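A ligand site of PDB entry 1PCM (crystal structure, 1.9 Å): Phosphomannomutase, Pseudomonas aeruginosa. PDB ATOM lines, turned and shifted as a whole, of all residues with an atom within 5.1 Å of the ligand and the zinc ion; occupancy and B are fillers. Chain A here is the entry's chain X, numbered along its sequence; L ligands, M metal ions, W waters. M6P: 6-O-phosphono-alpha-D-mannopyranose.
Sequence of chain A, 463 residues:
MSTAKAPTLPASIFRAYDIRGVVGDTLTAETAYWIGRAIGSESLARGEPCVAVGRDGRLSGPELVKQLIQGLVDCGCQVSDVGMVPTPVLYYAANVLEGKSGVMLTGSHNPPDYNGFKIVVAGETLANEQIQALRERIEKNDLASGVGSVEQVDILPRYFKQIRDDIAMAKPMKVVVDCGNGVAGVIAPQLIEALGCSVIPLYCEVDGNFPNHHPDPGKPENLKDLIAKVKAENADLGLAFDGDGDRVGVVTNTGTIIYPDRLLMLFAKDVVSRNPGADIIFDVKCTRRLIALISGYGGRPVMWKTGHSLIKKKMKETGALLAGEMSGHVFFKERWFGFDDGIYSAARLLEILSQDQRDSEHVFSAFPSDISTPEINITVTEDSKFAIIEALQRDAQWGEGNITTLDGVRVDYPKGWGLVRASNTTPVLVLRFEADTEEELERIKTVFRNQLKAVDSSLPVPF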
ATOM      1  N   TYR A  17      -2.102  21.317 -34.920  1.00  0.00           N
ATOM      2  CA  TYR A  17      -1.529  20.363 -33.950  1.00  0.00           C
ATOM      3  C   TYR A  17      -2.194  19.000 -33.986  1.00  0.00           C
ATOM      4  O   TYR A  17      -1.580  17.995 -33.595  1.00  0.00           O
ATOM      5  CB  TYR A  17      -1.623  20.887 -32.516  1.00  0.00           C
ATOM      6  CG  TYR A  17      -1.254  22.344 -32.281  1.00  0.00           C
ATOM      7  CD1 TYR A  17      -0.213  22.955 -32.965  1.00  0.00           C
ATOM      8  CD2 TYR A  17      -1.944  23.086 -31.336  1.00  0.00           C
ATOM      9  CE1 TYR A  17       0.127  24.287 -32.731  1.00  0.00           C
ATOM     10  CE2 TYR A  17      -1.631  24.430 -31.097  1.00  0.00           C
ATOM     11  CZ  TYR A  17      -0.597  25.018 -31.785  1.00  0.00           C
ATOM     12  OH  TYR A  17      -0.302  26.345 -31.543  1.00  0.00           O
ATOM     13  N   ASP A  18      -3.456  18.986 -34.416  1.00  0.00           N
ATOM     14  CA  ASP A  18      -4.316  17.821 -34.324  1.00  0.00           C
ATOM     15  C   ASP A  18      -5.611  18.047 -35.119  1.00  0.00           C
ATOM     16  O   ASP A  18      -5.723  19.038 -35.829  1.00  0.00           O
ATOM     17  CB  ASP A  18      -4.621  17.469 -32.852  1.00  0.00           C
ATOM     18  CG  ASP A  18      -5.013  18.681 -32.030  1.00  0.00           C
ATOM     19  OD1 ASP A  18      -5.937  19.399 -32.459  1.00  0.00           O
ATOM     20  OD2 ASP A  18      -4.467  18.939 -30.920  1.00  0.00           O
ATOM     21  N   SEP A 108     -10.056  17.297 -25.783  1.00  0.00           N
ATOM     22  CA  SEP A 108      -9.156  17.997 -24.857  1.00  0.00           C
ATOM     23  CB  SEP A 108      -8.163  18.879 -25.652  1.00  0.00           C
ATOM     24  OG  SEP A 108      -7.300  19.537 -24.745  1.00  0.00           O
ATOM     25  C   SEP A 108      -9.884  18.760 -23.727  1.00  0.00           C
ATOM     26  O   SEP A 108     -10.487  18.133 -22.860  1.00  0.00           O
ATOM     27  P   SEP A 108      -5.863  20.064 -25.232  1.00  0.00           P
ATOM     28  O1P SEP A 108      -6.030  21.656 -25.211  1.00  0.00           O
ATOM     29  O2P SEP A 108      -5.399  19.568 -26.687  1.00  0.00           O
ATOM     30  O3P SEP A 108      -4.766  19.691 -24.153  1.00  0.00           O
ATOM     31  N   HIS A 109      -9.843  20.106 -23.738  1.00  0.00           N
ATOM     32  CA  HIS A 109     -10.440  20.951 -22.688  1.00  0.00           C
ATOM     33  C   HIS A 109     -11.750  21.622 -23.144  1.00  0.00           C
ATOM     34  O   HIS A 109     -12.363  22.388 -22.381  1.00  0.00           O
ATOM     35  CB  HIS A 109      -9.449  22.023 -22.207  1.00  0.00           C
ATOM     36  CG  HIS A 109      -8.997  22.993 -23.281  1.00  0.00           C
ATOM     37  ND1 HIS A 109      -8.235  22.605 -24.358  1.00  0.00           N
ATOM     38  CD2 HIS A 109      -9.176  24.331 -23.393  1.00  0.00           C
ATOM     39  CE1 HIS A 109      -7.978  23.667 -25.118  1.00  0.00           C
ATOM     40  NE2 HIS A 109      -8.534  24.727 -24.556  1.00  0.00           N
ATOM     41  N   LYS A 118      -5.734  13.136 -31.764  1.00  0.00           N
ATOM     42  CA  LYS A 118      -4.329  13.431 -31.656  1.00  0.00           C
ATOM     43  C   LYS A 118      -3.600  12.177 -32.146  1.00  0.00           C
ATOM     44  O   LYS A 118      -3.942  11.042 -31.760  1.00  0.00           O
ATOM     45  CB  LYS A 118      -3.970  13.794 -30.216  1.00  0.00           C
ATOM     46  CG  LYS A 118      -4.641  15.066 -29.709  1.00  0.00           C
ATOM     47  CD  LYS A 118      -4.386  15.360 -28.235  1.00  0.00           C
ATOM     48  CE  LYS A 118      -4.991  16.682 -27.806  1.00  0.00           C
ATOM     49  NZ  LYS A 118      -4.663  17.018 -26.403  1.00  0.00           N
ATOM     50  N   ASP A 242      -6.688  18.830 -16.903  1.00  0.00           N
ATOM     51  CA  ASP A 242      -7.608  19.146 -17.989  1.00  0.00           C
ATOM     52  C   ASP A 242      -8.343  17.886 -18.407  1.00  0.00           C
ATOM     53  O   ASP A 242      -8.115  16.801 -17.855  1.00  0.00           O
ATOM     54  CB  ASP A 242      -6.908  19.866 -19.148  1.00  0.00           C
ATOM     55  CG  ASP A 242      -6.225  18.926 -20.137  1.00  0.00           C
ATOM     56  OD1 ASP A 242      -5.770  17.806 -19.755  1.00  0.00           O
ATOM     57  OD2 ASP A 242      -6.087  19.266 -21.315  1.00  0.00           O
ATOM     58  N   ASP A 244      -8.396  15.604 -20.742  1.00  0.00           N
ATOM     59  CA  ASP A 244      -7.758  14.372 -21.218  1.00  0.00           C
ATOM     60  C   ASP A 244      -6.451  14.032 -20.504  1.00  0.00           C
ATOM     61  O   ASP A 244      -5.807  13.039 -20.828  1.00  0.00           O
ATOM     62  CB  ASP A 244      -7.545  14.413 -22.734  1.00  0.00           C
ATOM     63  CG  ASP A 244      -6.611  15.535 -23.183  1.00  0.00           C
ATOM     64  OD1 ASP A 244      -5.898  15.367 -24.191  1.00  0.00           O
ATOM     65  OD2 ASP A 244      -6.559  16.631 -22.603  1.00  0.00           O
ATOM     66  N   GLY A 245      -6.076  14.851 -19.527  1.00  0.00           N
ATOM     67  CA  GLY A 245      -4.970  14.554 -18.637  1.00  0.00           C
ATOM     68  C   GLY A 245      -3.556  14.850 -19.104  1.00  0.00           C
ATOM     69  O   GLY A 245      -2.592  14.397 -18.465  1.00  0.00           O
ATOM     70  N   ASP A 246      -3.398  15.610 -20.189  1.00  0.00           N
ATOM     71  CA  ASP A 246      -2.059  16.010 -20.664  1.00  0.00           C
ATOM     72  C   ASP A 246      -1.606  17.380 -20.158  1.00  0.00           C
ATOM     73  O   ASP A 246      -0.487  17.825 -20.432  1.00  0.00           O
ATOM     74  CB  ASP A 246      -1.942  15.905 -22.193  1.00  0.00           C
ATOM     75  CG  ASP A 246      -2.951  16.735 -22.933  1.00  0.00           C
ATOM     76  OD1 ASP A 246      -3.737  17.494 -22.330  1.00  0.00           O
ATOM     77  OD2 ASP A 246      -3.030  16.695 -24.181  1.00  0.00           O
ATOM     78  N   ARG A 247      -2.483  18.028 -19.388  1.00  0.00           N
ATOM     79  CA  ARG A 247      -2.189  19.315 -18.771  1.00  0.00           C
ATOM     80  C   ARG A 247      -2.460  19.236 -17.282  1.00  0.00           C
ATOM     81  O   ARG A 247      -3.409  18.586 -16.844  1.00  0.00           O
ATOM     82  CB  ARG A 247      -3.044  20.416 -19.408  1.00  0.00           C
ATOM     83  N   LYS A 285       5.674  31.748 -25.070  1.00  0.00           N
ATOM     84  CA  LYS A 285       4.854  32.397 -24.033  1.00  0.00           C
ATOM     85  C   LYS A 285       5.470  32.382 -22.631  1.00  0.00           C
ATOM     86  O   LYS A 285       4.879  32.937 -21.709  1.00  0.00           O
ATOM     87  CB  LYS A 285       3.498  31.725 -23.932  1.00  0.00           C
ATOM     88  CG  LYS A 285       2.744  31.648 -25.199  1.00  0.00           C
ATOM     89  CD  LYS A 285       1.423  30.992 -24.940  1.00  0.00           C
ATOM     90  CE  LYS A 285       0.625  30.857 -26.193  1.00  0.00           C
ATOM     91  NZ  LYS A 285      -0.560  30.024 -25.935  1.00  0.00           N
ATOM     92  N   THR A 306       4.731  27.396 -29.699  1.00  0.00           N
ATOM     93  CA  THR A 306       3.573  26.860 -28.990  1.00  0.00           C
ATOM     94  C   THR A 306       2.981  25.707 -29.770  1.00  0.00           C
ATOM     95  O   THR A 306       2.977  25.719 -30.979  1.00  0.00           O
ATOM     96  CB  THR A 306       2.529  27.999 -28.867  1.00  0.00           C
ATOM     97  OG1 THR A 306       3.047  29.024 -27.993  1.00  0.00           O
ATOM     98  CG2 THR A 306       1.211  27.535 -28.226  1.00  0.00           C
ATOM     99  N   GLY A 307       2.486  24.688 -29.055  1.00  0.00           N
ATOM    100  CA  GLY A 307       1.703  23.610 -29.647  1.00  0.00           C
ATOM    101  C   GLY A 307       2.308  22.270 -29.307  1.00  0.00           C
ATOM    102  O   GLY A 307       3.456  22.051 -29.618  1.00  0.00           O
ATOM    103  N   HIS A 308       1.536  21.383 -28.695  1.00  0.00           N
ATOM    104  CA  HIS A 308       2.091  20.115 -28.193  1.00  0.00           C
ATOM    105  C   HIS A 308       2.859  19.311 -29.223  1.00  0.00           C
ATOM    106  O   HIS A 308       3.969  18.839 -28.956  1.00  0.00           O
ATOM    107  CB  HIS A 308       1.003  19.260 -27.544  1.00  0.00           C
ATOM    108  CG  HIS A 308      -0.005  18.688 -28.507  1.00  0.00           C
ATOM    109  ND1 HIS A 308      -0.327  17.350 -28.530  1.00  0.00           N
ATOM    110  CD2 HIS A 308      -0.712  19.264 -29.506  1.00  0.00           C
ATOM    111  CE1 HIS A 308      -1.239  17.133 -29.457  1.00  0.00           C
ATOM    112  NE2 HIS A 308      -1.481  18.272 -30.068  1.00  0.00           N
ATOM    113  N   GLU A 325       5.189  24.004 -21.908  1.00  0.00           N
ATOM    114  CA  GLU A 325       4.467  25.113 -22.506  1.00  0.00           C
ATOM    115  C   GLU A 325       3.759  25.908 -21.419  1.00  0.00           C
ATOM    116  O   GLU A 325       3.419  25.369 -20.368  1.00  0.00           O
ATOM    117  CB  GLU A 325       3.394  24.578 -23.414  1.00  0.00           C
ATOM    118  CG  GLU A 325       3.857  23.856 -24.644  1.00  0.00           C
ATOM    119  CD  GLU A 325       2.669  23.662 -25.538  1.00  0.00           C
ATOM    120  OE1 GLU A 325       2.339  24.615 -26.260  1.00  0.00           O
ATOM    121  OE2 GLU A 325       2.008  22.610 -25.404  1.00  0.00           O
ATOM    122  N   SER A 327       0.767  26.677 -21.464  1.00  0.00           N
ATOM    123  CA  SER A 327      -0.565  26.065 -21.350  1.00  0.00           C
ATOM    124  C   SER A 327      -0.621  24.914 -20.340  1.00  0.00           C
ATOM    125  O   SER A 327      -1.688  24.402 -20.069  1.00  0.00           O
ATOM    126  CB  SER A 327      -1.037  25.562 -22.717  1.00  0.00           C
ATOM    127  OG  SER A 327      -0.123  24.602 -23.226  1.00  0.00           O
ATOM    128  N   HIS A 329       1.231  21.959 -20.592  1.00  0.00           N
ATOM    129  CA  HIS A 329       1.736  20.691 -21.141  1.00  0.00           C
ATOM    130  C   HIS A 329       3.188  20.589 -20.733  1.00  0.00           C
ATOM    131  O   HIS A 329       3.974  21.480 -21.048  1.00  0.00           O
ATOM    132  CB  HIS A 329       1.593  20.610 -22.685  1.00  0.00           C
ATOM    133  CG  HIS A 329       0.175  20.579 -23.137  1.00  0.00           C
ATOM    134  ND1 HIS A 329      -0.529  19.419 -23.306  1.00  0.00           N
ATOM    135  CD2 HIS A 329      -0.693  21.577 -23.431  1.00  0.00           C
ATOM    136  CE1 HIS A 329      -1.774  19.698 -23.661  1.00  0.00           C
ATOM    137  NE2 HIS A 329      -1.898  21.008 -23.735  1.00  0.00           N
ATOM    138  N   GLU A 375      -2.355  35.818 -20.454  1.00  0.00           N
ATOM    139  CA  GLU A 375      -2.553  35.739 -21.896  1.00  0.00           C
ATOM    140  C   GLU A 375      -3.673  36.713 -22.342  1.00  0.00           C
ATOM    141  O   GLU A 375      -4.760  36.733 -21.764  1.00  0.00           O
ATOM    142  CB  GLU A 375      -2.867  34.289 -22.332  1.00  0.00           C
ATOM    143  CG  GLU A 375      -1.962  33.739 -23.430  1.00  0.00           C
ATOM    144  CD  GLU A 375      -1.630  32.258 -23.297  1.00  0.00           C
ATOM    145  OE1 GLU A 375      -1.159  31.820 -22.221  1.00  0.00           O
ATOM    146  OE2 GLU A 375      -1.801  31.517 -24.294  1.00  0.00           O
ATOM    147  N   ARG A 421       1.515  36.544 -31.316  1.00  0.00           N
ATOM    148  CA  ARG A 421       1.499  35.449 -32.281  1.00  0.00           C
ATOM    149  C   ARG A 421       0.057  35.073 -32.636  1.00  0.00           C
ATOM    150  O   ARG A 421      -0.885  35.433 -31.946  1.00  0.00           O
ATOM    151  CB  ARG A 421       2.233  34.249 -31.680  1.00  0.00           C
ATOM    152  CG  ARG A 421       1.601  33.727 -30.398  1.00  0.00           C
ATOM    153  CD  ARG A 421       2.193  32.426 -29.881  1.00  0.00           C
ATOM    154  NE  ARG A 421       1.805  31.231 -30.642  1.00  0.00           N
ATOM    155  CZ  ARG A 421       0.647  30.603 -30.551  1.00  0.00           C
ATOM    156  NH1 ARG A 421      -0.312  31.030 -29.746  1.00  0.00           N
ATOM    157  NH2 ARG A 421       0.464  29.487 -31.245  1.00  0.00           N
ATOM    158  N   ALA A 422      -0.102  34.346 -33.730  1.00  0.00           N
ATOM    159  CA  ALA A 422      -1.384  33.782 -34.114  1.00  0.00           C
ATOM    160  C   ALA A 422      -1.658  32.474 -33.385  1.00  0.00           C
ATOM    161  O   ALA A 422      -0.828  31.570 -33.385  1.00  0.00           O
ATOM    162  CB  ALA A 422      -1.402  33.556 -35.606  1.00  0.00           C
ATOM    163  N   SER A 423      -2.851  32.362 -32.791  1.00  0.00           N
ATOM    164  CA  SER A 423      -3.347  31.082 -32.302  1.00  0.00           C
ATOM    165  C   SER A 423      -3.549  30.116 -33.459  1.00  0.00           C
ATOM    166  O   SER A 423      -3.995  30.520 -34.536  1.00  0.00           O
ATOM    167  CB  SER A 423      -4.692  31.278 -31.587  1.00  0.00           C
ATOM    168  OG  SER A 423      -5.268  30.046 -31.196  1.00  0.00           O
ATOM    169  N   ASN A 424      -3.209  28.850 -33.236  1.00  0.00           N
ATOM    170  CA  ASN A 424      -3.560  27.767 -34.148  1.00  0.00           C
ATOM    171  C   ASN A 424      -4.742  26.899 -33.664  1.00  0.00           C
ATOM    172  O   ASN A 424      -4.948  25.765 -34.154  1.00  0.00           O
ATOM    173  CB  ASN A 424      -2.341  26.856 -34.387  1.00  0.00           C
ATOM    174  CG  ASN A 424      -1.125  27.611 -34.904  1.00  0.00           C
ATOM    175  OD1 ASN A 424      -0.090  27.675 -34.244  1.00  0.00           O
ATOM    176  ND2 ASN A 424      -1.250  28.173 -36.083  1.00  0.00           N
ATOM    177  N   THR A 425      -5.497  27.382 -32.665  1.00  0.00           N
ATOM    178  CA  THR A 425      -6.740  26.711 -32.225  1.00  0.00           C
ATOM    179  C   THR A 425      -7.974  27.589 -32.317  1.00  0.00           C
ATOM    180  O   THR A 425      -9.108  27.080 -32.271  1.00  0.00           O
ATOM    181  CB  THR A 425      -6.613  26.123 -30.797  1.00  0.00           C
ATOM    182  OG1 THR A 425      -6.363  27.136 -29.829  1.00  0.00           O
ATOM    183  CG2 THR A 425      -5.420  25.166 -30.679  1.00  0.00           C
ATOM    184  N   THR A 426      -7.761  28.902 -32.484  1.00  0.00           N
ATOM    185  CA  THR A 426      -8.816  29.912 -32.584  1.00  0.00           C
ATOM    186  C   THR A 426      -8.394  31.020 -33.554  1.00  0.00           C
ATOM    187  O   THR A 426      -7.212  31.170 -33.849  1.00  0.00           O
ATOM    188  CB  THR A 426      -9.090  30.543 -31.207  1.00  0.00           C
ATOM    189  OG1 THR A 426      -7.861  31.006 -30.635  1.00  0.00           O
ATOM    190  CG2 THR A 426      -9.601  29.501 -30.230  1.00  0.00           C
ATOM    191  N   VAL A 430      -2.648  36.216 -29.980  1.00  0.00           N
ATOM    192  CA  VAL A 430      -2.333  35.968 -28.593  1.00  0.00           C
ATOM    193  C   VAL A 430      -1.113  36.820 -28.224  1.00  0.00           C
ATOM    194  O   VAL A 430      -0.100  36.801 -28.933  1.00  0.00           O
ATOM    195  CB  VAL A 430      -1.970  34.469 -28.395  1.00  0.00           C
ATOM    196  CG1 VAL A 430      -1.650  34.176 -26.956  1.00  0.00           C
ATOM    197  CG2 VAL A 430      -3.088  33.559 -28.903  1.00  0.00           C
HETATM  198  C1  M6P L   1      -3.857  23.432 -26.738  1.00  0.00           C
HETATM  199  C2  M6P L   1      -2.654  22.535 -26.955  1.00  0.00           C
HETATM  200  C3  M6P L   1      -1.373  23.181 -26.357  1.00  0.00           C
HETATM  201  C4  M6P L   1      -1.216  24.673 -26.691  1.00  0.00           C
HETATM  202  C5  M6P L   1      -2.551  25.425 -26.498  1.00  0.00           C
HETATM  203  C6  M6P L   1      -2.382  26.854 -27.006  1.00  0.00           C
HETATM  204  O1  M6P L   1      -4.169  23.467 -25.346  1.00  0.00           O
HETATM  205  O2  M6P L   1      -2.458  22.307 -28.376  1.00  0.00           O
HETATM  206  O3  M6P L   1      -0.248  22.492 -26.877  1.00  0.00           O
HETATM  207  O4  M6P L   1      -0.228  25.230 -25.848  1.00  0.00           O
HETATM  208  O5  M6P L   1      -3.582  24.779 -27.237  1.00  0.00           O
HETATM  209  O6  M6P L   1      -2.477  26.823 -28.479  1.00  0.00           O
HETATM  210  P   M6P L   1      -2.622  28.206 -29.300  1.00  0.00           P
HETATM  211  O1P M6P L   1      -1.869  29.234 -28.533  1.00  0.00           O
HETATM  212  O2P M6P L   1      -4.071  28.573 -29.410  1.00  0.00           O
HETATM  213  O3P M6P L   1      -2.075  27.981 -30.676  1.00  0.00           O
HETATM  214 ZN    ZN M   1      -5.413  18.229 -22.817  1.00  0.00          ZN
HETATM  215  O   HOH W   1      -4.688  20.669 -29.099  1.00  0.00           O
HETATM  216  O   HOH W   2       1.472  27.415 -24.543  1.00  0.00           O
HETATM  217  O   HOH W   3      -5.205  29.975 -27.192  1.00  0.00           O
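The side-chain amino group of Lys 118 is in salt-bridge range of the side-chain carboxylate of Asp 246. The backbone NH of Asp 242 lies within hydrogen-bond range of the backbone carbonyl oxygen of Arg 247, 3.3 Å away. O3P of SEP 108 lies close to NE2 of His 329. O of Thr 306 is in hydrogen-bond range of OH of Tyr 17. N of Thr 425 lies within hydrogen-bond range of OG of Ser 423. OG of Ser 423 lies within hydrogen-bond range of OG1 of Thr 426 (2.8 Å). The backbone NH of Val 430 is in hydrogen-bond range of the backbone carbonyl oxygen of Arg 421, 2.8 Å away. OE1 of Glu 325 is in hydrogen-bond range of N of Gly 307, 2.8 Å away.
His 109 touches the ligand (CE1 to O1, 3.8 Å). Thr 306 touches the ligand (CG2 to O1P, 3.5 Å). Gly 307 touches the ligand. His 329 touches the ligand (CD2 to C3, 3.4 Å). Within 4 Å of the ligand: Tyr 17, SEP 108, His 109, Lys 285, Thr 306, Gly 307, His 308, Glu 325, Ser 327, His 329, Arg 421, Ser 423, Asn 424 and Thr 425.
Water W1 lies within hydrogen-bond range of the side-chain carboxylate of Asp 18 (2.5 Å), O2P of SEP 108 (2.7 Å) and an oxygen (O2) of the ligand (2.9 Å). Water W2 lies within hydrogen-bond range of an oxygen (O4) of the ligand (3.1 Å), the backbone NH (N) of Ser 327 (3.2 Å) and the side-chain carboxylate (OE1) of Glu 325 (3.4 Å).
O1P of SEP 108 sits at hydrogen-bond distance from an oxygen (O1) of the ligand (2.6 Å). An oxygen (O3P) of the ligand is in hydrogen-bond range of the side-chain hydroxyl of Tyr 17 (2.6 Å). OG of Ser 423 is in hydrogen-bond range of O2P of the ligand, at 2.6 Å. An oxygen (O1P) of the ligand is in salt-bridge range of the guanidinium group of Arg 421, at 2.7 Å. O4 of the ligand lies within hydrogen-bond range of OE1 of Glu 325 (2.7 Å). The side-chain hydroxyl (OG) of Ser 327 sits at hydrogen-bond distance from an oxygen (O4) of the ligand (2.7 Å). O2P of the ligand sits at hydrogen-bond distance from OG1 of Thr 425. The backbone NH of His 308 sits at hydrogen-bond distance from an oxygen (O3) of the ligand (2.8 Å). The backbone NH of Asn 424 sits at hydrogen-bond distance from an oxygen (O3P) of the ligand (2.9 Å). NZ of Lys 285 lies within salt-bridge range of O1P of the ligand (3.0 Å).
The zinc ion is bound by OD1 of Asp 246 (1.9 Å), OD2 of Asp 242 (1.9 Å), OD2 of Asp 244 (2.0 Å) and O3P of SEP 108 (2.1 Å).
Lys 118 touches the zinc ion (NZ to ZN, 3.9 Å).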
